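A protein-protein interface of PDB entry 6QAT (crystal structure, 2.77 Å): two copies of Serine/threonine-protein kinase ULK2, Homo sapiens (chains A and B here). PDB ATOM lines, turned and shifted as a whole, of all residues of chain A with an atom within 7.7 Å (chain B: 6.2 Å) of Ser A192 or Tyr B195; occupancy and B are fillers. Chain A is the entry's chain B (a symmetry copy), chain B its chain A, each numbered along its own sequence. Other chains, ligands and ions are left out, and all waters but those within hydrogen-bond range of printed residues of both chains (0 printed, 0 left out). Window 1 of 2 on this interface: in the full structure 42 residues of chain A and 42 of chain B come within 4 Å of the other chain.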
ATOM      1  N   ARG A 167     -15.811  -9.177   7.928  1.00  0.00           N
ATOM      2  CA  ARG A 167     -14.365  -8.969   7.697  1.00  0.00           C
ATOM      3  C   ARG A 167     -14.156  -8.474   6.265  1.00  0.00           C
ATOM      4  O   ARG A 167     -15.027  -8.741   5.414  1.00  0.00           O
ATOM      5  CB  ARG A 167     -13.589 -10.253   8.020  1.00  0.00           C
ATOM      6  CG  ARG A 167     -13.222 -11.106   6.821  1.00  0.00           C
ATOM      7  CD  ARG A 167     -12.231 -12.188   7.228  1.00  0.00           C
ATOM      8  NE  ARG A 167     -11.866 -13.064   6.123  1.00  0.00           N
ATOM      9  CZ  ARG A 167     -10.918 -12.805   5.230  1.00  0.00           C
ATOM     10  NH1 ARG A 167     -10.225 -11.694   5.298  1.00  0.00           N
ATOM     11  NH2 ARG A 167     -10.682 -13.661   4.258  1.00  0.00           N
ATOM     12  N   LEU A 169     -12.033  -8.284   2.784  1.00  0.00           N
ATOM     13  CA  LEU A 169     -11.114  -9.057   1.903  1.00  0.00           C
ATOM     14  C   LEU A 169      -9.897  -8.205   1.590  1.00  0.00           C
ATOM     15  O   LEU A 169     -10.083  -7.057   1.158  1.00  0.00           O
ATOM     16  CB  LEU A 169     -11.852  -9.445   0.628  1.00  0.00           C
ATOM     17  CG  LEU A 169     -12.835 -10.597   0.777  1.00  0.00           C
ATOM     18  CD1 LEU A 169     -13.776 -10.649  -0.415  1.00  0.00           C
ATOM     19  CD2 LEU A 169     -12.090 -11.931   0.952  1.00  0.00           C
ATOM     20  N   ALA A 186       3.238 -16.859   7.134  1.00  0.00           N
ATOM     21  CA  ALA A 186       2.920 -18.314   7.141  1.00  0.00           C
ATOM     22  C   ALA A 186       2.176 -18.697   5.876  1.00  0.00           C
ATOM     23  O   ALA A 186       1.234 -18.013   5.478  1.00  0.00           O
ATOM     24  CB  ALA A 186       2.104 -18.676   8.349  1.00  0.00           C
ATOM     25  N   PRO A 187       2.545 -19.841   5.247  1.00  0.00           N
ATOM     26  CA  PRO A 187       1.917 -20.277   4.005  1.00  0.00           C
ATOM     27  C   PRO A 187       0.398 -20.486   4.117  1.00  0.00           C
ATOM     28  O   PRO A 187      -0.295 -20.196   3.159  1.00  0.00           O
ATOM     29  CB  PRO A 187       2.624 -21.618   3.691  1.00  0.00           C
ATOM     30  CG  PRO A 187       3.967 -21.517   4.420  1.00  0.00           C
ATOM     31  CD  PRO A 187       3.667 -20.706   5.654  1.00  0.00           C
ATOM     32  N   GLU A 188      -0.080 -21.023   5.246  1.00  0.00           N
ATOM     33  CA  GLU A 188      -1.536 -21.277   5.487  1.00  0.00           C
ATOM     34  C   GLU A 188      -2.320 -19.954   5.383  1.00  0.00           C
ATOM     35  O   GLU A 188      -3.466 -19.986   4.867  1.00  0.00           O
ATOM     36  CB  GLU A 188      -1.792 -21.954   6.843  1.00  0.00           C
ATOM     37  CG  GLU A 188      -1.308 -21.171   8.040  1.00  0.00           C
ATOM     38  CD  GLU A 188       0.056 -21.637   8.563  1.00  0.00           C
ATOM     39  OE1 GLU A 188       0.908 -22.017   7.731  1.00  0.00           O
ATOM     40  OE2 GLU A 188       0.279 -21.584   9.784  1.00  0.00           O
ATOM     41  N   VAL A 189      -1.697 -18.831   5.785  1.00  0.00           N
ATOM     42  CA  VAL A 189      -2.308 -17.468   5.753  1.00  0.00           C
ATOM     43  C   VAL A 189      -2.284 -16.943   4.313  1.00  0.00           C
ATOM     44  O   VAL A 189      -3.298 -16.397   3.858  1.00  0.00           O
ATOM     45  CB  VAL A 189      -1.599 -16.500   6.712  1.00  0.00           C
ATOM     46  CG1 VAL A 189      -2.219 -15.121   6.651  1.00  0.00           C
ATOM     47  CG2 VAL A 189      -1.582 -17.023   8.147  1.00  0.00           C
ATOM     48  N   ILE A 190      -1.159 -17.074   3.646  1.00  0.00           N
ATOM     49  CA  ILE A 190      -0.974 -16.650   2.227  1.00  0.00           C
ATOM     50  C   ILE A 190      -2.071 -17.295   1.370  1.00  0.00           C
ATOM     51  O   ILE A 190      -2.671 -16.581   0.527  1.00  0.00           O
ATOM     52  CB  ILE A 190       0.423 -17.036   1.733  1.00  0.00           C
ATOM     53  CG1 ILE A 190       1.514 -16.264   2.471  1.00  0.00           C
ATOM     54  CG2 ILE A 190       0.525 -16.871   0.223  1.00  0.00           C
ATOM     55  CD1 ILE A 190       1.634 -14.840   2.054  1.00  0.00           C
ATOM     56  N   MET A 191      -2.308 -18.593   1.576  1.00  0.00           N
ATOM     57  CA  MET A 191      -3.064 -19.461   0.654  1.00  0.00           C
ATOM     58  C   MET A 191      -4.557 -19.294   0.920  1.00  0.00           C
ATOM     59  O   MET A 191      -5.340 -19.306  -0.062  1.00  0.00           O
ATOM     60  CB  MET A 191      -2.673 -20.927   0.850  1.00  0.00           C
ATOM     61  CG  MET A 191      -1.299 -21.262   0.322  1.00  0.00           C
ATOM     62  SD  MET A 191      -1.000 -23.007   0.380  1.00  0.00           S
ATOM     63  CE  MET A 191      -0.561 -23.241   2.099  1.00  0.00           C
ATOM     64  N   SER A 192      -4.923 -19.071   2.192  1.00  0.00           N
ATOM     65  CA  SER A 192      -6.315 -19.034   2.688  1.00  0.00           C
ATOM     66  C   SER A 192      -6.923 -17.639   2.475  1.00  0.00           C
ATOM     67  O   SER A 192      -8.072 -17.435   2.884  1.00  0.00           O
ATOM     68  CB  SER A 192      -6.376 -19.443   4.137  1.00  0.00           C
ATOM     69  OG  SER A 192      -5.884 -18.404   4.981  1.00  0.00           O
ATOM     70  N   GLN A 193      -6.155 -16.707   1.913  1.00  0.00           N
ATOM     71  CA  GLN A 193      -6.666 -15.425   1.362  1.00  0.00           C
ATOM     72  C   GLN A 193      -7.892 -15.726   0.490  1.00  0.00           C
ATOM     73  O   GLN A 193      -7.797 -16.638  -0.342  1.00  0.00           O
ATOM     74  CB  GLN A 193      -5.552 -14.717   0.573  1.00  0.00           C
ATOM     75  CG  GLN A 193      -5.913 -13.305   0.111  1.00  0.00           C
ATOM     76  CD  GLN A 193      -4.771 -12.322   0.279  1.00  0.00           C
ATOM     77  OE1 GLN A 193      -4.607 -11.709   1.333  1.00  0.00           O
ATOM     78  NE2 GLN A 193      -3.980 -12.158  -0.771  1.00  0.00           N
ATOM     79  N   HIS A 194      -9.029 -15.076   0.774  1.00  0.00           N
ATOM     80  CA  HIS A 194     -10.277 -15.116  -0.048  1.00  0.00           C
ATOM     81  C   HIS A 194     -11.040 -16.451   0.146  1.00  0.00           C
ATOM     82  O   HIS A 194     -12.046 -16.637  -0.540  1.00  0.00           O
ATOM     83  CB  HIS A 194      -9.960 -14.883  -1.531  1.00  0.00           C
ATOM     84  CG  HIS A 194      -9.722 -13.453  -1.883  1.00  0.00           C
ATOM     85  ND1 HIS A 194     -10.208 -12.884  -3.053  1.00  0.00           N
ATOM     86  CD2 HIS A 194      -8.995 -12.487  -1.268  1.00  0.00           C
ATOM     87  CE1 HIS A 194      -9.798 -11.632  -3.134  1.00  0.00           C
ATOM     88  NE2 HIS A 194      -9.053 -11.364  -2.050  1.00  0.00           N
ATOM     89  N   TYR A 195     -10.614 -17.301   1.088  1.00  0.00           N
ATOM     90  CA  TYR A 195     -11.146 -18.682   1.288  1.00  0.00           C
ATOM     91  C   TYR A 195     -12.639 -18.627   1.660  1.00  0.00           C
ATOM     92  O   TYR A 195     -13.381 -19.576   1.297  1.00  0.00           O
ATOM     93  CB  TYR A 195     -10.340 -19.448   2.350  1.00  0.00           C
ATOM     94  CG  TYR A 195     -10.780 -19.210   3.765  1.00  0.00           C
ATOM     95  CD1 TYR A 195     -10.256 -18.167   4.508  1.00  0.00           C
ATOM     96  CD2 TYR A 195     -11.754 -19.990   4.350  1.00  0.00           C
ATOM     97  CE1 TYR A 195     -10.681 -17.907   5.797  1.00  0.00           C
ATOM     98  CE2 TYR A 195     -12.184 -19.756   5.648  1.00  0.00           C
ATOM     99  CZ  TYR A 195     -11.640 -18.706   6.376  1.00  0.00           C
ATOM    100  OH  TYR A 195     -12.055 -18.427   7.654  1.00  0.00           O
ATOM    101  N   ASP A 196     -13.068 -17.560   2.358  1.00  0.00           N
ATOM    102  CA  ASP A 196     -14.461 -17.400   2.857  1.00  0.00           C
ATOM    103  C   ASP A 196     -15.200 -16.337   2.017  1.00  0.00           C
ATOM    104  O   ASP A 196     -16.311 -15.988   2.383  1.00  0.00           O
ATOM    105  CB  ASP A 196     -14.474 -17.081   4.349  1.00  0.00           C
ATOM    106  CG  ASP A 196     -13.612 -15.892   4.754  1.00  0.00           C
ATOM    107  OD1 ASP A 196     -12.643 -15.577   4.000  1.00  0.00           O
ATOM    108  OD2 ASP A 196     -13.902 -15.291   5.832  1.00  0.00           O
ATOM    109  N   ALA A 197     -14.668 -16.007   0.840  1.00  0.00           N
ATOM    110  CA  ALA A 197     -15.167 -14.935  -0.050  1.00  0.00           C
ATOM    111  C   ALA A 197     -16.639 -15.169  -0.384  1.00  0.00           C
ATOM    112  O   ALA A 197     -17.304 -14.196  -0.792  1.00  0.00           O
ATOM    113  CB  ALA A 197     -14.331 -14.869  -1.303  1.00  0.00           C
ATOM    114  N   GLN A 260     -16.727 -24.121  -1.826  1.00  0.00           N
ATOM    115  CA  GLN A 260     -16.902 -22.730  -2.347  1.00  0.00           C
ATOM    116  C   GLN A 260     -16.493 -22.680  -3.822  1.00  0.00           C
ATOM    117  O   GLN A 260     -17.112 -21.892  -4.585  1.00  0.00           O
ATOM    118  CB  GLN A 260     -16.057 -21.734  -1.539  1.00  0.00           C
ATOM    119  CG  GLN A 260     -14.585 -22.134  -1.386  1.00  0.00           C
ATOM    120  CD  GLN A 260     -14.317 -22.891  -0.103  1.00  0.00           C
ATOM    121  OE1 GLN A 260     -15.016 -23.848   0.240  1.00  0.00           O
ATOM    122  NE2 GLN A 260     -13.300 -22.455   0.632  1.00  0.00           N
ATOM    123  N   ARG B 134       0.380 -12.876  13.051  1.00  0.00           N
ATOM    124  CA  ARG B 134       0.094 -13.310  11.654  1.00  0.00           C
ATOM    125  C   ARG B 134       0.982 -12.560  10.659  1.00  0.00           C
ATOM    126  O   ARG B 134       1.033 -12.976   9.504  1.00  0.00           O
ATOM    127  CB  ARG B 134      -1.366 -13.094  11.302  1.00  0.00           C
ATOM    128  CG  ARG B 134      -2.310 -13.991  12.070  1.00  0.00           C
ATOM    129  CD  ARG B 134      -3.512 -14.333  11.262  1.00  0.00           C
ATOM    130  NE  ARG B 134      -4.300 -13.177  10.921  1.00  0.00           N
ATOM    131  CZ  ARG B 134      -5.179 -13.145   9.936  1.00  0.00           C
ATOM    132  NH1 ARG B 134      -5.309 -14.194   9.128  1.00  0.00           N
ATOM    133  NH2 ARG B 134      -5.872 -12.040   9.713  1.00  0.00           N
ATOM    134  N   ARG B 167      -5.388 -11.287  15.145  1.00  0.00           N
ATOM    135  CA  ARG B 167      -6.779 -11.721  15.328  1.00  0.00           C
ATOM    136  C   ARG B 167      -6.859 -12.635  16.552  1.00  0.00           C
ATOM    137  O   ARG B 167      -5.817 -13.199  16.948  1.00  0.00           O
ATOM    138  CB  ARG B 167      -7.303 -12.386  14.052  1.00  0.00           C
ATOM    139  CG  ARG B 167      -7.140 -13.894  14.011  1.00  0.00           C
ATOM    140  CD  ARG B 167      -7.785 -14.486  12.780  1.00  0.00           C
ATOM    141  NE  ARG B 167      -7.682 -15.932  12.780  1.00  0.00           N
ATOM    142  CZ  ARG B 167      -8.521 -16.751  13.397  1.00  0.00           C
ATOM    143  NH1 ARG B 167      -9.558 -16.271  14.058  1.00  0.00           N
ATOM    144  NH2 ARG B 167      -8.328 -18.051  13.339  1.00  0.00           N
ATOM    145  N   LEU B 169      -8.365 -15.915  18.483  1.00  0.00           N
ATOM    146  CA  LEU B 169      -8.873 -17.306  18.286  1.00  0.00           C
ATOM    147  C   LEU B 169     -10.227 -17.445  18.974  1.00  0.00           C
ATOM    148  O   LEU B 169     -10.307 -17.120  20.165  1.00  0.00           O
ATOM    149  CB  LEU B 169      -7.860 -18.298  18.866  1.00  0.00           C
ATOM    150  CG  LEU B 169      -6.641 -18.560  18.001  1.00  0.00           C
ATOM    151  CD1 LEU B 169      -5.528 -19.214  18.806  1.00  0.00           C
ATOM    152  CD2 LEU B 169      -7.018 -19.413  16.802  1.00  0.00           C
ATOM    153  N   MET B 191     -15.001 -24.711   9.619  1.00  0.00           N
ATOM    154  CA  MET B 191     -13.950 -25.757   9.605  1.00  0.00           C
ATOM    155  C   MET B 191     -12.571 -25.103   9.742  1.00  0.00           C
ATOM    156  O   MET B 191     -11.716 -25.701  10.407  1.00  0.00           O
ATOM    157  CB  MET B 191     -14.017 -26.585   8.314  1.00  0.00           C
ATOM    158  CG  MET B 191     -15.259 -27.516   8.254  1.00  0.00           C
ATOM    159  SD  MET B 191     -15.348 -28.606   6.768  1.00  0.00           S
ATOM    160  CE  MET B 191     -15.505 -27.382   5.463  1.00  0.00           C
ATOM    161  N   SER B 192     -12.413 -23.871   9.236  1.00  0.00           N
ATOM    162  CA  SER B 192     -11.121 -23.126   9.164  1.00  0.00           C
ATOM    163  C   SER B 192     -10.823 -22.403  10.493  1.00  0.00           C
ATOM    164  O   SER B 192      -9.789 -21.722  10.567  1.00  0.00           O
ATOM    165  CB  SER B 192     -11.129 -22.146   8.009  1.00  0.00           C
ATOM    166  OG  SER B 192     -11.978 -21.041   8.283  1.00  0.00           O
ATOM    167  N   GLN B 193     -11.723 -22.503  11.465  1.00  0.00           N
ATOM    168  CA  GLN B 193     -11.468 -22.169  12.896  1.00  0.00           C
ATOM    169  C   GLN B 193     -10.106 -22.758  13.314  1.00  0.00           C
ATOM    170  O   GLN B 193      -9.872 -23.930  13.030  1.00  0.00           O
ATOM    171  CB  GLN B 193     -12.624 -22.712  13.760  1.00  0.00           C
ATOM    172  CG  GLN B 193     -12.573 -22.282  15.220  1.00  0.00           C
ATOM    173  CD  GLN B 193     -13.955 -22.065  15.806  1.00  0.00           C
ATOM    174  OE1 GLN B 193     -14.538 -20.987  15.686  1.00  0.00           O
ATOM    175  NE2 GLN B 193     -14.480 -23.087  16.473  1.00  0.00           N
ATOM    176  N   HIS B 194      -9.215 -21.925  13.849  1.00  0.00           N
ATOM    177  CA  HIS B 194      -7.914 -22.313  14.475  1.00  0.00           C
ATOM    178  C   HIS B 194      -6.867 -22.697  13.408  1.00  0.00           C
ATOM    179  O   HIS B 194      -5.773 -23.114  13.806  1.00  0.00           O
ATOM    180  CB  HIS B 194      -8.110 -23.455  15.470  1.00  0.00           C
ATOM    181  CG  HIS B 194      -8.634 -23.021  16.797  1.00  0.00           C
ATOM    182  ND1 HIS B 194      -8.062 -23.436  18.000  1.00  0.00           N
ATOM    183  CD2 HIS B 194      -9.663 -22.212  17.127  1.00  0.00           C
ATOM    184  CE1 HIS B 194      -8.746 -22.926  19.005  1.00  0.00           C
ATOM    185  NE2 HIS B 194      -9.735 -22.173  18.500  1.00  0.00           N
ATOM    186  N   TYR B 195      -7.167 -22.499  12.115  1.00  0.00           N
ATOM    187  CA  TYR B 195      -6.328 -22.975  10.978  1.00  0.00           C
ATOM    188  C   TYR B 195      -4.956 -22.274  11.009  1.00  0.00           C
ATOM    189  O   TYR B 195      -3.951 -22.881  10.562  1.00  0.00           O
ATOM    190  CB  TYR B 195      -7.049 -22.763   9.642  1.00  0.00           C
ATOM    191  CG  TYR B 195      -6.834 -21.426   9.019  1.00  0.00           C
ATOM    192  CD1 TYR B 195      -7.677 -20.371   9.295  1.00  0.00           C
ATOM    193  CD2 TYR B 195      -5.746 -21.186   8.192  1.00  0.00           C
ATOM    194  CE1 TYR B 195      -7.461 -19.112   8.752  1.00  0.00           C
ATOM    195  CE2 TYR B 195      -5.514 -19.931   7.651  1.00  0.00           C
ATOM    196  CZ  TYR B 195      -6.380 -18.896   7.927  1.00  0.00           C
ATOM    197  OH  TYR B 195      -6.173 -17.675   7.372  1.00  0.00           O
ATOM    198  N   ASP B 196      -4.912 -21.031  11.506  1.00  0.00           N
ATOM    199  CA  ASP B 196      -3.690 -20.187  11.536  1.00  0.00           C
ATOM    200  C   ASP B 196      -3.180 -20.071  12.976  1.00  0.00           C
ATOM    201  O   ASP B 196      -2.269 -19.292  13.202  1.00  0.00           O
ATOM    202  CB  ASP B 196      -3.943 -18.818  10.901  1.00  0.00           C
ATOM    203  CG  ASP B 196      -5.141 -18.078  11.455  1.00  0.00           C
ATOM    204  OD1 ASP B 196      -6.030 -18.736  11.983  1.00  0.00           O
ATOM    205  OD2 ASP B 196      -5.192 -16.847  11.297  1.00  0.00           O
ATOM    206  N   ALA B 197      -3.605 -20.974  13.845  1.00  0.00           N
ATOM    207  CA  ALA B 197      -3.224 -21.015  15.275  1.00  0.00           C
ATOM    208  C   ALA B 197      -1.702 -21.071  15.421  1.00  0.00           C
ATOM    209  O   ALA B 197      -1.214 -20.691  16.497  1.00  0.00           O
ATOM    210  CB  ALA B 197      -3.881 -22.182  15.957  1.00  0.00           C
ATOM    211  N   LYS B 198      -0.980 -21.524  14.383  1.00  0.00           N
ATOM    212  CA  LYS B 198       0.485 -21.782  14.456  1.00  0.00           C
ATOM    213  C   LYS B 198       1.230 -20.894  13.459  1.00  0.00           C
ATOM    214  O   LYS B 198       2.443 -21.050  13.348  1.00  0.00           O
ATOM    215  CB  LYS B 198       0.782 -23.250  14.189  1.00  0.00           C
ATOM    216  CG  LYS B 198       0.652 -24.169  15.393  1.00  0.00           C
ATOM    217  CD  LYS B 198       0.753 -25.661  15.027  1.00  0.00           C
ATOM    218  CE  LYS B 198       0.520 -26.576  16.205  1.00  0.00           C
ATOM    219  NZ  LYS B 198       0.823 -27.982  15.861  1.00  0.00           N
ATOM    220  N   ALA B 199       0.544 -19.920  12.858  1.00  0.00           N
ATOM    221  CA  ALA B 199       1.081 -19.029  11.794  1.00  0.00           C
ATOM    222  C   ALA B 199       2.322 -18.274  12.302  1.00  0.00           C
ATOM    223  O   ALA B 199       3.235 -18.054  11.509  1.00  0.00           O
ATOM    224  CB  ALA B 199       0.010 -18.078  11.330  1.00  0.00           C
ATOM    225  N   ARG B 227       2.229 -16.935  -3.689  1.00  0.00           N
ATOM    226  CA  ARG B 227       0.887 -17.562  -3.516  1.00  0.00           C
ATOM    227  C   ARG B 227       0.903 -18.938  -4.188  1.00  0.00           C
ATOM    228  O   ARG B 227       0.614 -19.944  -3.501  1.00  0.00           O
ATOM    229  CB  ARG B 227      -0.228 -16.682  -4.104  1.00  0.00           C
ATOM    230  CG  ARG B 227      -1.630 -17.197  -3.794  1.00  0.00           C
ATOM    231  CD  ARG B 227      -2.719 -16.166  -3.951  1.00  0.00           C
ATOM    232  NE  ARG B 227      -3.961 -16.622  -3.322  1.00  0.00           N
ATOM    233  CZ  ARG B 227      -5.134 -15.988  -3.396  1.00  0.00           C
ATOM    234  NH1 ARG B 227      -6.200 -16.499  -2.804  1.00  0.00           N
ATOM    235  NH2 ARG B 227      -5.240 -14.856  -4.069  1.00  0.00           N
ATOM    236  N   GLN B 260       0.812 -27.042   9.022  1.00  0.00           N
ATOM    237  CA  GLN B 260       0.750 -26.659  10.466  1.00  0.00           C
ATOM    238  C   GLN B 260       0.579 -27.902  11.331  1.00  0.00           C
ATOM    239  O   GLN B 260       1.101 -27.902  12.458  1.00  0.00           O
ATOM    240  CB  GLN B 260      -0.399 -25.682  10.730  1.00  0.00           C
ATOM    241  CG  GLN B 260      -1.742 -26.114  10.160  1.00  0.00           C
ATOM    242  CD  GLN B 260      -2.003 -25.508   8.799  1.00  0.00           C
ATOM    243  OE1 GLN B 260      -1.165 -25.573   7.898  1.00  0.00           O
ATOM    244  NE2 GLN B 260      -3.196 -24.954   8.623  1.00  0.00           N
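OG of Ser B192 sits at hydrogen-bond distance from OH of Tyr A195. OG of Ser A192 sits at hydrogen-bond distance from OH of Tyr B195. NH1 of Arg B227 lies within hydrogen-bond range of O of Gln A193, at 2.9 Å.
Ser A192 touches Tyr B195, and with the chains exchanged Tyr A195 touches Ser B192. Of the 10 pairs that touch across the chains among the printed residues, 2 have their exchanged pair printed and touching as well.
Among the printed residues, pairs that only touch across the chains: Glu A188 with Ala B199 (3.3 Å), Ala A186 with Ala B199 (3.4 Å), Glu A188 with Tyr B195 (3.5 Å), Val A189 with Ala B199 (3.7 Å), Glu A188 with Gln B260 (3.8 Å), Ile A190 with Arg B227 (3.8 Å) and Glu A188 with Lys B198 (3.9 Å).
The side-chain amide nitrogen (NE2) of Gln B260 is in hydrogen-bond range of the backbone carbonyl oxygen (O) of Tyr B195, at 2.9 Å. NZ of Lys B198 lies within hydrogen-bond range of O of Gln B260. The backbone carbonyl oxygen (O) of Glu A188 is in hydrogen-bond range of the side-chain hydroxyl (OG) of Ser A192, at 2.9 Å. OG of Ser A192 is in hydrogen-bond range of O of Val A189 (3.5 Å). NE2 of Gln A260 lies within hydrogen-bond range of O of Tyr A195, 3.0 Å away.
Of chain B, only Tyr B195 (2.5 Å) comes within 4 Å of Ser A192. Of the printed residues of chain A, Tyr B195 touches Glu A188 and Ser A192. Of the printed residues of chain A, Arg B227 touches Ile A190 and Gln A193. Printed residues of chain B within 4 Å of Glu A188: Tyr B195 (3.5 Å), Lys B198 (3.9 Å), Ala B199 (3.3 Å) and Gln B260 (3.8 Å). Printed residues of chain A within 4 Å of Ala B199: Ala A186 (3.4 Å), Glu A188 (3.3 Å) and Val A189 (3.7 Å). Printed residues of chain A within 4 Å of Lys B198: Glu A188 (3.9 Å). Gln A260 touches none of the printed residues of chain B. Met A191 touches none of the printed residues of chain B. The nearest printed residue of chain A that does not touch Arg B227 is Met A191 (4.02 Å).
Of the 15 printed residues of chain A, 7 touch a printed residue of chain B. Hydrophobic or aromatic side chains of chain A that line the printed part of chain B: Ala A186, Val A189, Ile A190 and Tyr A195. Of the 14 printed residues of chain B, 6 touch a printed residue of chain A. Printed residues of chain B that touch a printed residue of chain A: Ser B192, Tyr B195, Lys B198, Ala B199, Arg B227 and Gln B260. Hydrophobic or aromatic side chains of chain B that line the printed part of chain A: Tyr B195 and Ala B199. Among the printed residues, no Asp or Glu carboxylate lies within 4 Å of a Lys or Arg side-chain nitrogen of the other chain.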
